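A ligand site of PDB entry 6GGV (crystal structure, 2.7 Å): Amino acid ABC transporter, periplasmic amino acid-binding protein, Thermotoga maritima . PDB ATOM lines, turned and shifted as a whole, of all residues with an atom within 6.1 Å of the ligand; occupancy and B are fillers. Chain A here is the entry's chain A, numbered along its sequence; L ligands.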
ATOM      1  N   SER A  16     -25.130 -13.656   0.300  1.00  0.00           N
ATOM      2  CA  SER A  16     -25.185 -12.267  -0.110  1.00  0.00           C
ATOM      3  C   SER A  16     -25.792 -12.300  -1.486  1.00  0.00           C
ATOM      4  O   SER A  16     -25.129 -12.584  -2.457  1.00  0.00           O
ATOM      5  CB  SER A  16     -23.787 -11.640  -0.187  1.00  0.00           C
ATOM      6  OG  SER A  16     -23.826 -10.306  -0.661  1.00  0.00           O
ATOM      7  N   ALA A  17     -27.079 -11.971  -1.522  1.00  0.00           N
ATOM      8  CA  ALA A  17     -27.915 -12.010  -2.718  1.00  0.00           C
ATOM      9  C   ALA A  17     -27.630 -10.928  -3.747  1.00  0.00           C
ATOM     10  O   ALA A  17     -28.562 -10.292  -4.278  1.00  0.00           O
ATOM     11  CB  ALA A  17     -29.380 -11.969  -2.299  1.00  0.00           C
ATOM     12  N   ASP A  18     -26.359 -10.721  -4.062  1.00  0.00           N
ATOM     13  CA  ASP A  18     -25.983  -9.711  -5.060  1.00  0.00           C
ATOM     14  C   ASP A  18     -25.022 -10.285  -6.090  1.00  0.00           C
ATOM     15  O   ASP A  18     -24.216  -9.567  -6.652  1.00  0.00           O
ATOM     16  CB  ASP A  18     -25.385  -8.475  -4.363  1.00  0.00           C
ATOM     17  CG  ASP A  18     -24.039  -8.770  -3.673  1.00  0.00           C
ATOM     18  OD1 ASP A  18     -23.759  -9.943  -3.360  1.00  0.00           O
ATOM     19  OD2 ASP A  18     -23.283  -7.806  -3.441  1.00  0.00           O
ATOM     20  N   PHE A  19     -25.153 -11.566  -6.364  1.00  0.00           N
ATOM     21  CA  PHE A  19     -24.139 -12.328  -7.056  1.00  0.00           C
ATOM     22  C   PHE A  19     -24.859 -13.329  -7.976  1.00  0.00           C
ATOM     23  O   PHE A  19     -24.846 -14.560  -7.704  1.00  0.00           O
ATOM     24  CB  PHE A  19     -23.335 -13.047  -5.974  1.00  0.00           C
ATOM     25  CG  PHE A  19     -21.963 -13.565  -6.408  1.00  0.00           C
ATOM     26  CD1 PHE A  19     -20.953 -12.698  -6.803  1.00  0.00           C
ATOM     27  CD2 PHE A  19     -21.652 -14.920  -6.280  1.00  0.00           C
ATOM     28  CE1 PHE A  19     -19.700 -13.178  -7.144  1.00  0.00           C
ATOM     29  CE2 PHE A  19     -20.397 -15.398  -6.611  1.00  0.00           C
ATOM     30  CZ  PHE A  19     -19.418 -14.518  -7.046  1.00  0.00           C
ATOM     31  N   GLU A  23     -26.657 -16.224  -6.361  1.00  0.00           N
ATOM     32  CA  GLU A  23     -27.659 -15.682  -5.431  1.00  0.00           C
ATOM     33  C   GLU A  23     -27.987 -14.214  -5.703  1.00  0.00           C
ATOM     34  O   GLU A  23     -27.101 -13.375  -5.672  1.00  0.00           O
ATOM     35  CB  GLU A  23     -27.241 -15.852  -3.977  1.00  0.00           C
ATOM     36  CG  GLU A  23     -25.878 -15.324  -3.637  1.00  0.00           C
ATOM     37  CD  GLU A  23     -24.810 -16.377  -3.652  1.00  0.00           C
ATOM     38  OE1 GLU A  23     -25.103 -17.558  -3.405  1.00  0.00           O
ATOM     39  OE2 GLU A  23     -23.636 -16.028  -3.866  1.00  0.00           O
ATOM     40  N   ASP A  35     -27.079 -21.259  -6.179  1.00  0.00           N
ATOM     41  CA  ASP A  35     -26.692 -21.541  -4.822  1.00  0.00           C
ATOM     42  C   ASP A  35     -27.900 -21.866  -3.968  1.00  0.00           C
ATOM     43  O   ASP A  35     -27.814 -22.713  -3.082  1.00  0.00           O
ATOM     44  CB  ASP A  35     -25.897 -20.392  -4.199  1.00  0.00           C
ATOM     45  CG  ASP A  35     -24.387 -20.576  -4.328  1.00  0.00           C
ATOM     46  OD1 ASP A  35     -23.902 -21.629  -4.781  1.00  0.00           O
ATOM     47  OD2 ASP A  35     -23.667 -19.646  -3.940  1.00  0.00           O
ATOM     48  N   PHE A  57     -21.404  -9.908   2.327  1.00  0.00           N
ATOM     49  CA  PHE A  57     -20.427 -10.998   2.158  1.00  0.00           C
ATOM     50  C   PHE A  57     -19.449 -11.162   3.342  1.00  0.00           C
ATOM     51  O   PHE A  57     -19.310 -12.246   3.906  1.00  0.00           O
ATOM     52  CB  PHE A  57     -19.672 -10.822   0.835  1.00  0.00           C
ATOM     53  CG  PHE A  57     -18.716 -11.940   0.521  1.00  0.00           C
ATOM     54  CD1 PHE A  57     -19.176 -13.179   0.113  1.00  0.00           C
ATOM     55  CD2 PHE A  57     -17.342 -11.730   0.592  1.00  0.00           C
ATOM     56  CE1 PHE A  57     -18.291 -14.209  -0.187  1.00  0.00           C
ATOM     57  CE2 PHE A  57     -16.450 -12.742   0.287  1.00  0.00           C
ATOM     58  CZ  PHE A  57     -16.928 -14.003  -0.103  1.00  0.00           C
ATOM     59  N   LEU A  60     -20.396 -13.306   6.443  1.00  0.00           N
ATOM     60  CA  LEU A  60     -20.600 -14.754   6.440  1.00  0.00           C
ATOM     61  C   LEU A  60     -19.737 -15.502   7.457  1.00  0.00           C
ATOM     62  O   LEU A  60     -20.258 -16.114   8.357  1.00  0.00           O
ATOM     63  CB  LEU A  60     -20.381 -15.326   5.036  1.00  0.00           C
ATOM     64  CG  LEU A  60     -21.257 -14.659   4.026  1.00  0.00           C
ATOM     65  CD1 LEU A  60     -20.784 -14.989   2.619  1.00  0.00           C
ATOM     66  CD2 LEU A  60     -22.721 -15.054   4.253  1.00  0.00           C
ATOM     67  N   SER A  74     -22.586 -19.272  -0.725  1.00  0.00           N
ATOM     68  CA  SER A  74     -22.586 -17.910  -1.283  1.00  0.00           C
ATOM     69  C   SER A  74     -21.394 -17.614  -2.190  1.00  0.00           C
ATOM     70  O   SER A  74     -20.602 -16.702  -1.892  1.00  0.00           O
ATOM     71  CB  SER A  74     -22.660 -16.868  -0.148  1.00  0.00           C
ATOM     72  OG  SER A  74     -22.543 -15.523  -0.638  1.00  0.00           O
ATOM     73  N   GLY A  75     -21.294 -18.362  -3.304  1.00  0.00           N
ATOM     74  CA  GLY A  75     -20.191 -18.244  -4.267  1.00  0.00           C
ATOM     75  C   GLY A  75     -18.819 -18.078  -3.640  1.00  0.00           C
ATOM     76  O   GLY A  75     -17.987 -17.307  -4.124  1.00  0.00           O
ATOM     77  N   MET A  76     -18.572 -18.806  -2.555  1.00  0.00           N
ATOM     78  CA  MET A  76     -17.396 -18.539  -1.754  1.00  0.00           C
ATOM     79  C   MET A  76     -16.241 -19.392  -2.192  1.00  0.00           C
ATOM     80  O   MET A  76     -16.327 -20.614  -2.165  1.00  0.00           O
ATOM     81  CB  MET A  76     -17.666 -18.723  -0.265  1.00  0.00           C
ATOM     82  CG  MET A  76     -16.452 -18.397   0.569  1.00  0.00           C
ATOM     83  SD  MET A  76     -16.779 -17.896   2.261  1.00  0.00           S
ATOM     84  CE  MET A  76     -17.056 -19.504   2.981  1.00  0.00           C
ATOM     85  N   THR A  77     -15.164 -18.704  -2.573  1.00  0.00           N
ATOM     86  CA  THR A  77     -13.913 -19.334  -2.987  1.00  0.00           C
ATOM     87  C   THR A  77     -13.254 -20.075  -1.827  1.00  0.00           C
ATOM     88  O   THR A  77     -13.167 -19.555  -0.706  1.00  0.00           O
ATOM     89  CB  THR A  77     -12.951 -18.264  -3.569  1.00  0.00           C
ATOM     90  OG1 THR A  77     -13.536 -17.704  -4.756  1.00  0.00           O
ATOM     91  CG2 THR A  77     -11.582 -18.847  -3.959  1.00  0.00           C
ATOM     92  N   ILE A  78     -12.818 -21.297  -2.104  1.00  0.00           N
ATOM     93  CA  ILE A  78     -11.941 -22.047  -1.202  1.00  0.00           C
ATOM     94  C   ILE A  78     -10.524 -21.444  -1.174  1.00  0.00           C
ATOM     95  O   ILE A  78      -9.709 -21.656  -2.099  1.00  0.00           O
ATOM     96  CB  ILE A  78     -11.871 -23.553  -1.606  1.00  0.00           C
ATOM     97  CG1 ILE A  78     -13.231 -24.228  -1.484  1.00  0.00           C
ATOM     98  CG2 ILE A  78     -10.845 -24.273  -0.783  1.00  0.00           C
ATOM     99  CD1 ILE A  78     -13.395 -25.526  -2.305  1.00  0.00           C
ATOM    100  N   THR A  79     -10.232 -20.681  -0.122  1.00  0.00           N
ATOM    101  CA  THR A  79      -8.862 -20.172   0.118  1.00  0.00           C
ATOM    102  C   THR A  79      -8.244 -20.864   1.316  1.00  0.00           C
ATOM    103  O   THR A  79      -8.966 -21.331   2.207  1.00  0.00           O
ATOM    104  CB  THR A  79      -8.843 -18.662   0.373  1.00  0.00           C
ATOM    105  OG1 THR A  79      -9.589 -18.380   1.553  1.00  0.00           O
ATOM    106  CG2 THR A  79      -9.505 -17.931  -0.784  1.00  0.00           C
ATOM    107  N   ARG A  82      -9.114 -18.815   4.514  1.00  0.00           N
ATOM    108  CA  ARG A  82     -10.423 -19.095   5.045  1.00  0.00           C
ATOM    109  C   ARG A  82     -10.465 -20.506   5.608  1.00  0.00           C
ATOM    110  O   ARG A  82     -11.227 -20.767   6.547  1.00  0.00           O
ATOM    111  CB  ARG A  82     -11.469 -18.953   3.968  1.00  0.00           C
ATOM    112  CG  ARG A  82     -11.779 -17.539   3.643  1.00  0.00           C
ATOM    113  CD  ARG A  82     -12.628 -17.449   2.414  1.00  0.00           C
ATOM    114  NE  ARG A  82     -12.575 -16.093   1.870  1.00  0.00           N
ATOM    115  CZ  ARG A  82     -13.131 -15.727   0.707  1.00  0.00           C
ATOM    116  NH1 ARG A  82     -13.789 -16.608  -0.040  1.00  0.00           N
ATOM    117  NH2 ARG A  82     -13.016 -14.479   0.309  1.00  0.00           N
ATOM    118  N   GLN A  97     -11.168 -14.024 -11.290  1.00  0.00           N
ATOM    119  CA  GLN A  97     -11.337 -12.571 -11.376  1.00  0.00           C
ATOM    120  C   GLN A  97     -11.236 -12.067 -12.831  1.00  0.00           C
ATOM    121  O   GLN A  97     -10.352 -12.530 -13.594  1.00  0.00           O
ATOM    122  CB  GLN A  97     -10.290 -11.841 -10.524  1.00  0.00           C
ATOM    123  CG  GLN A  97     -10.278 -12.208  -9.052  1.00  0.00           C
ATOM    124  CD  GLN A  97     -11.651 -12.060  -8.421  1.00  0.00           C
ATOM    125  OE1 GLN A  97     -12.173 -10.961  -8.323  1.00  0.00           O
ATOM    126  NE2 GLN A  97     -12.241 -13.177  -7.999  1.00  0.00           N
ATOM    127  N   GLN A 123     -15.625  -5.695  -3.795  1.00  0.00           N
ATOM    128  CA  GLN A 123     -16.513  -6.002  -2.673  1.00  0.00           C
ATOM    129  C   GLN A 123     -15.610  -6.396  -1.505  1.00  0.00           C
ATOM    130  O   GLN A 123     -14.872  -7.364  -1.621  1.00  0.00           O
ATOM    131  CB  GLN A 123     -17.535  -7.114  -3.031  1.00  0.00           C
ATOM    132  CG  GLN A 123     -18.346  -7.689  -1.838  1.00  0.00           C
ATOM    133  CD  GLN A 123     -19.461  -8.677  -2.247  1.00  0.00           C
ATOM    134  OE1 GLN A 123     -19.212  -9.800  -2.692  1.00  0.00           O
ATOM    135  NE2 GLN A 123     -20.711  -8.244  -2.042  1.00  0.00           N
ATOM    136  N   GLY A 125     -13.652  -7.920   1.386  1.00  0.00           N
ATOM    137  CA  GLY A 125     -13.482  -9.280   1.877  1.00  0.00           C
ATOM    138  C   GLY A 125     -13.456 -10.371   0.821  1.00  0.00           C
ATOM    139  O   GLY A 125     -13.284 -11.567   1.134  1.00  0.00           O
ATOM    140  N   THR A 126     -13.630  -9.985  -0.445  1.00  0.00           N
ATOM    141  CA  THR A 126     -13.614 -10.996  -1.505  1.00  0.00           C
ATOM    142  C   THR A 126     -12.206 -11.219  -1.941  1.00  0.00           C
ATOM    143  O   THR A 126     -11.292 -10.507  -1.497  1.00  0.00           O
ATOM    144  CB  THR A 126     -14.468 -10.649  -2.774  1.00  0.00           C
ATOM    145  OG1 THR A 126     -13.976  -9.452  -3.383  1.00  0.00           O
ATOM    146  CG2 THR A 126     -15.903 -10.503  -2.422  1.00  0.00           C
ATOM    147  N   THR A 127     -12.067 -12.199  -2.819  1.00  0.00           N
ATOM    148  CA  THR A 127     -10.820 -12.542  -3.454  1.00  0.00           C
ATOM    149  C   THR A 127     -10.384 -11.467  -4.453  1.00  0.00           C
ATOM    150  O   THR A 127      -9.192 -11.258  -4.664  1.00  0.00           O
ATOM    151  CB  THR A 127     -10.917 -13.961  -4.128  1.00  0.00           C
ATOM    152  OG1 THR A 127     -12.108 -14.056  -4.929  1.00  0.00           O
ATOM    153  CG2 THR A 127     -10.973 -15.043  -3.081  1.00  0.00           C
ATOM    154  N   GLY A 128     -11.342 -10.776  -5.064  1.00  0.00           N
ATOM    155  CA  GLY A 128     -11.041  -9.588  -5.879  1.00  0.00           C
ATOM    156  C   GLY A 128     -10.433  -8.482  -5.025  1.00  0.00           C
ATOM    157  O   GLY A 128      -9.430  -7.894  -5.395  1.00  0.00           O
ATOM    158  N   PHE A 146     -22.088  -5.502  -4.674  1.00  0.00           N
ATOM    159  CA  PHE A 146     -21.612  -5.386  -6.066  1.00  0.00           C
ATOM    160  C   PHE A 146     -22.547  -4.458  -6.841  1.00  0.00           C
ATOM    161  O   PHE A 146     -22.189  -3.874  -7.886  1.00  0.00           O
ATOM    162  CB  PHE A 146     -21.566  -6.742  -6.784  1.00  0.00           C
ATOM    163  CG  PHE A 146     -20.300  -7.520  -6.543  1.00  0.00           C
ATOM    164  CD1 PHE A 146     -19.082  -7.053  -7.004  1.00  0.00           C
ATOM    165  CD2 PHE A 146     -20.341  -8.738  -5.874  1.00  0.00           C
ATOM    166  CE1 PHE A 146     -17.919  -7.761  -6.782  1.00  0.00           C
ATOM    167  CE2 PHE A 146     -19.163  -9.463  -5.650  1.00  0.00           C
ATOM    168  CZ  PHE A 146     -17.948  -8.979  -6.094  1.00  0.00           C
ATOM    169  N   ASP A 164     -15.443 -12.056  -9.748  1.00  0.00           N
ATOM    170  CA  ASP A 164     -15.488 -13.353 -10.422  1.00  0.00           C
ATOM    171  C   ASP A 164     -16.068 -13.263 -11.836  1.00  0.00           C
ATOM    172  O   ASP A 164     -16.962 -12.451 -12.099  1.00  0.00           O
ATOM    173  CB  ASP A 164     -16.313 -14.320  -9.571  1.00  0.00           C
ATOM    174  CG  ASP A 164     -15.771 -14.473  -8.160  1.00  0.00           C
ATOM    175  OD1 ASP A 164     -15.174 -13.498  -7.618  1.00  0.00           O
ATOM    176  OD2 ASP A 164     -15.939 -15.565  -7.589  1.00  0.00           O
ATOM    177  N   GLU A 188     -10.124 -20.107  -9.287  1.00  0.00           N
ATOM    178  CA  GLU A 188     -10.830 -20.261  -8.017  1.00  0.00           C
ATOM    179  C   GLU A 188     -11.831 -21.363  -8.133  1.00  0.00           C
ATOM    180  O   GLU A 188     -12.278 -21.680  -9.240  1.00  0.00           O
ATOM    181  CB  GLU A 188     -11.514 -18.942  -7.660  1.00  0.00           C
ATOM    182  CG  GLU A 188     -10.555 -17.765  -7.831  1.00  0.00           C
ATOM    183  CD  GLU A 188     -11.038 -16.469  -7.251  1.00  0.00           C
ATOM    184  OE1 GLU A 188     -12.235 -16.405  -6.888  1.00  0.00           O
ATOM    185  OE2 GLU A 188     -10.193 -15.530  -7.152  1.00  0.00           O
ATOM    186  N   TYR A 190     -15.341 -22.490  -5.847  1.00  0.00           N
ATOM    187  CA  TYR A 190     -16.277 -22.283  -4.738  1.00  0.00           C
ATOM    188  C   TYR A 190     -16.511 -23.548  -3.907  1.00  0.00           C
ATOM    189  O   TYR A 190     -16.609 -24.656  -4.446  1.00  0.00           O
ATOM    190  CB  TYR A 190     -17.635 -21.764  -5.223  1.00  0.00           C
ATOM    191  CG  TYR A 190     -17.596 -20.584  -6.173  1.00  0.00           C
ATOM    192  CD1 TYR A 190     -16.526 -19.671  -6.123  1.00  0.00           C
ATOM    193  CD2 TYR A 190     -18.625 -20.351  -7.084  1.00  0.00           C
ATOM    194  CE1 TYR A 190     -16.459 -18.591  -6.985  1.00  0.00           C
ATOM    195  CE2 TYR A 190     -18.570 -19.277  -7.944  1.00  0.00           C
ATOM    196  CZ  TYR A 190     -17.476 -18.384  -7.893  1.00  0.00           C
ATOM    197  OH  TYR A 190     -17.370 -17.268  -8.727  1.00  0.00           O
HETATM  198  N1  LIG L   1     -15.738 -16.311  -4.669  1.00  0.00           N
HETATM  199  C1  LIG L   1     -15.322 -14.953  -4.341  1.00  0.00           C
HETATM  200  C2  LIG L   1     -14.910 -14.883  -2.871  1.00  0.00           C
HETATM  201  O1  LIG L   1     -15.027 -15.878  -2.141  1.00  0.00           O
HETATM  202  C3  LIG L   1     -16.451 -13.940  -4.659  1.00  0.00           C
HETATM  203  C4  LIG L   1     -17.394 -13.654  -3.513  1.00  0.00           C
HETATM  204  C5  LIG L   1     -18.801 -13.947  -3.872  1.00  0.00           C
HETATM  205  N2  LIG L   1     -19.669 -12.842  -3.475  1.00  0.00           N
HETATM  206  C6  LIG L   1     -20.958 -12.926  -3.223  1.00  0.00           C
HETATM  207  N3  LIG L   1     -21.594 -11.829  -2.880  1.00  0.00           N
HETATM  208  N4  LIG L   1     -21.620 -14.083  -3.286  1.00  0.00           N
HETATM  209  O2  LIG L   1     -14.438 -13.860  -2.381  1.00  0.00           O
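The guanidinium group (NH1) of Arg 82 is in salt-bridge range of an oxygen (O1) of the ligand, at 2.5 Å.
The side-chain carboxylate (OD1) of Asp 18 lies within salt-bridge range of a nitrogen (N3) of the ligand.
OG of Ser 16 sits close to N3 of the ligand (3.5 Å).
The backbone carbonyl oxygen of Gly 75 is in hydrogen-bond range of a nitrogen (N1) of the ligand.
OE2 of Glu 23 is in salt-bridge range of N4 of the ligand, at 2.9 Å.
An oxygen (O2) of the ligand sits close to the side-chain hydroxyl (OG1) of Thr 127 (3.5 Å).
N3 of the ligand is in hydrogen-bond range of OE1 of Gln 123 (3.1 Å).
OG1 of Thr 77 lies within hydrogen-bond range of N1 of the ligand, 2.6 Å away.
The backbone NH (N) of Thr 77 lies within hydrogen-bond range of an oxygen (O1) of the ligand (2.9 Å).
An oxygen (O2) of the ligand sits at hydrogen-bond distance from the backbone NH (N) of Thr 127 (2.9 Å).
N4 of the ligand lies within hydrogen-bond range of O of Ser 74 (3.1 Å).
OD2 of Asp 164 lies within salt-bridge range of N1 of the ligand (3.0 Å).
A nitrogen (N4) of the ligand lies within hydrogen-bond range of the side-chain hydroxyl (OG) of Ser 74 (3.2 Å).
OE2 of Glu 23 lies close to OG of Ser 74 (3.4 Å).
The side-chain hydroxyl (OG1) of Thr 126 lies within hydrogen-bond range of the backbone carbonyl oxygen (O) of Gln 123, 2.9 Å away.
OD1 of Asp 164 is in hydrogen-bond range of NE2 of Gln 97, at 3.0 Å.
The backbone NH of Ser 16 lies within hydrogen-bond range of the side-chain hydroxyl of Ser 74 (3.3 Å).
OE1 of Glu 188 lies within hydrogen-bond range of OG1 of Thr 77, at 2.8 Å.
The side-chain carboxylate (OD2) of Asp 35 lies close to the side-chain carboxylate (OE1) of Glu 23 (2.6 Å).
OG1 of Thr 126 lies close to N of Gly 128.
OD2 of Asp 164 is in hydrogen-bond range of OH of Tyr 190, 2.5 Å away.
Residues that only touch the ligand: Phe 19, Phe 57, Met 76, Thr 126 and Tyr 190.
Hydrophobic or aromatic side chains that line the ligand: Phe 19, Phe 57, Met 76 and Tyr 190.
Of the 25 residues printed, 15 come within 4 Å of the ligand.
The nearest printed residue that does not touch the ligand is Phe 146 (4.1 Å).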
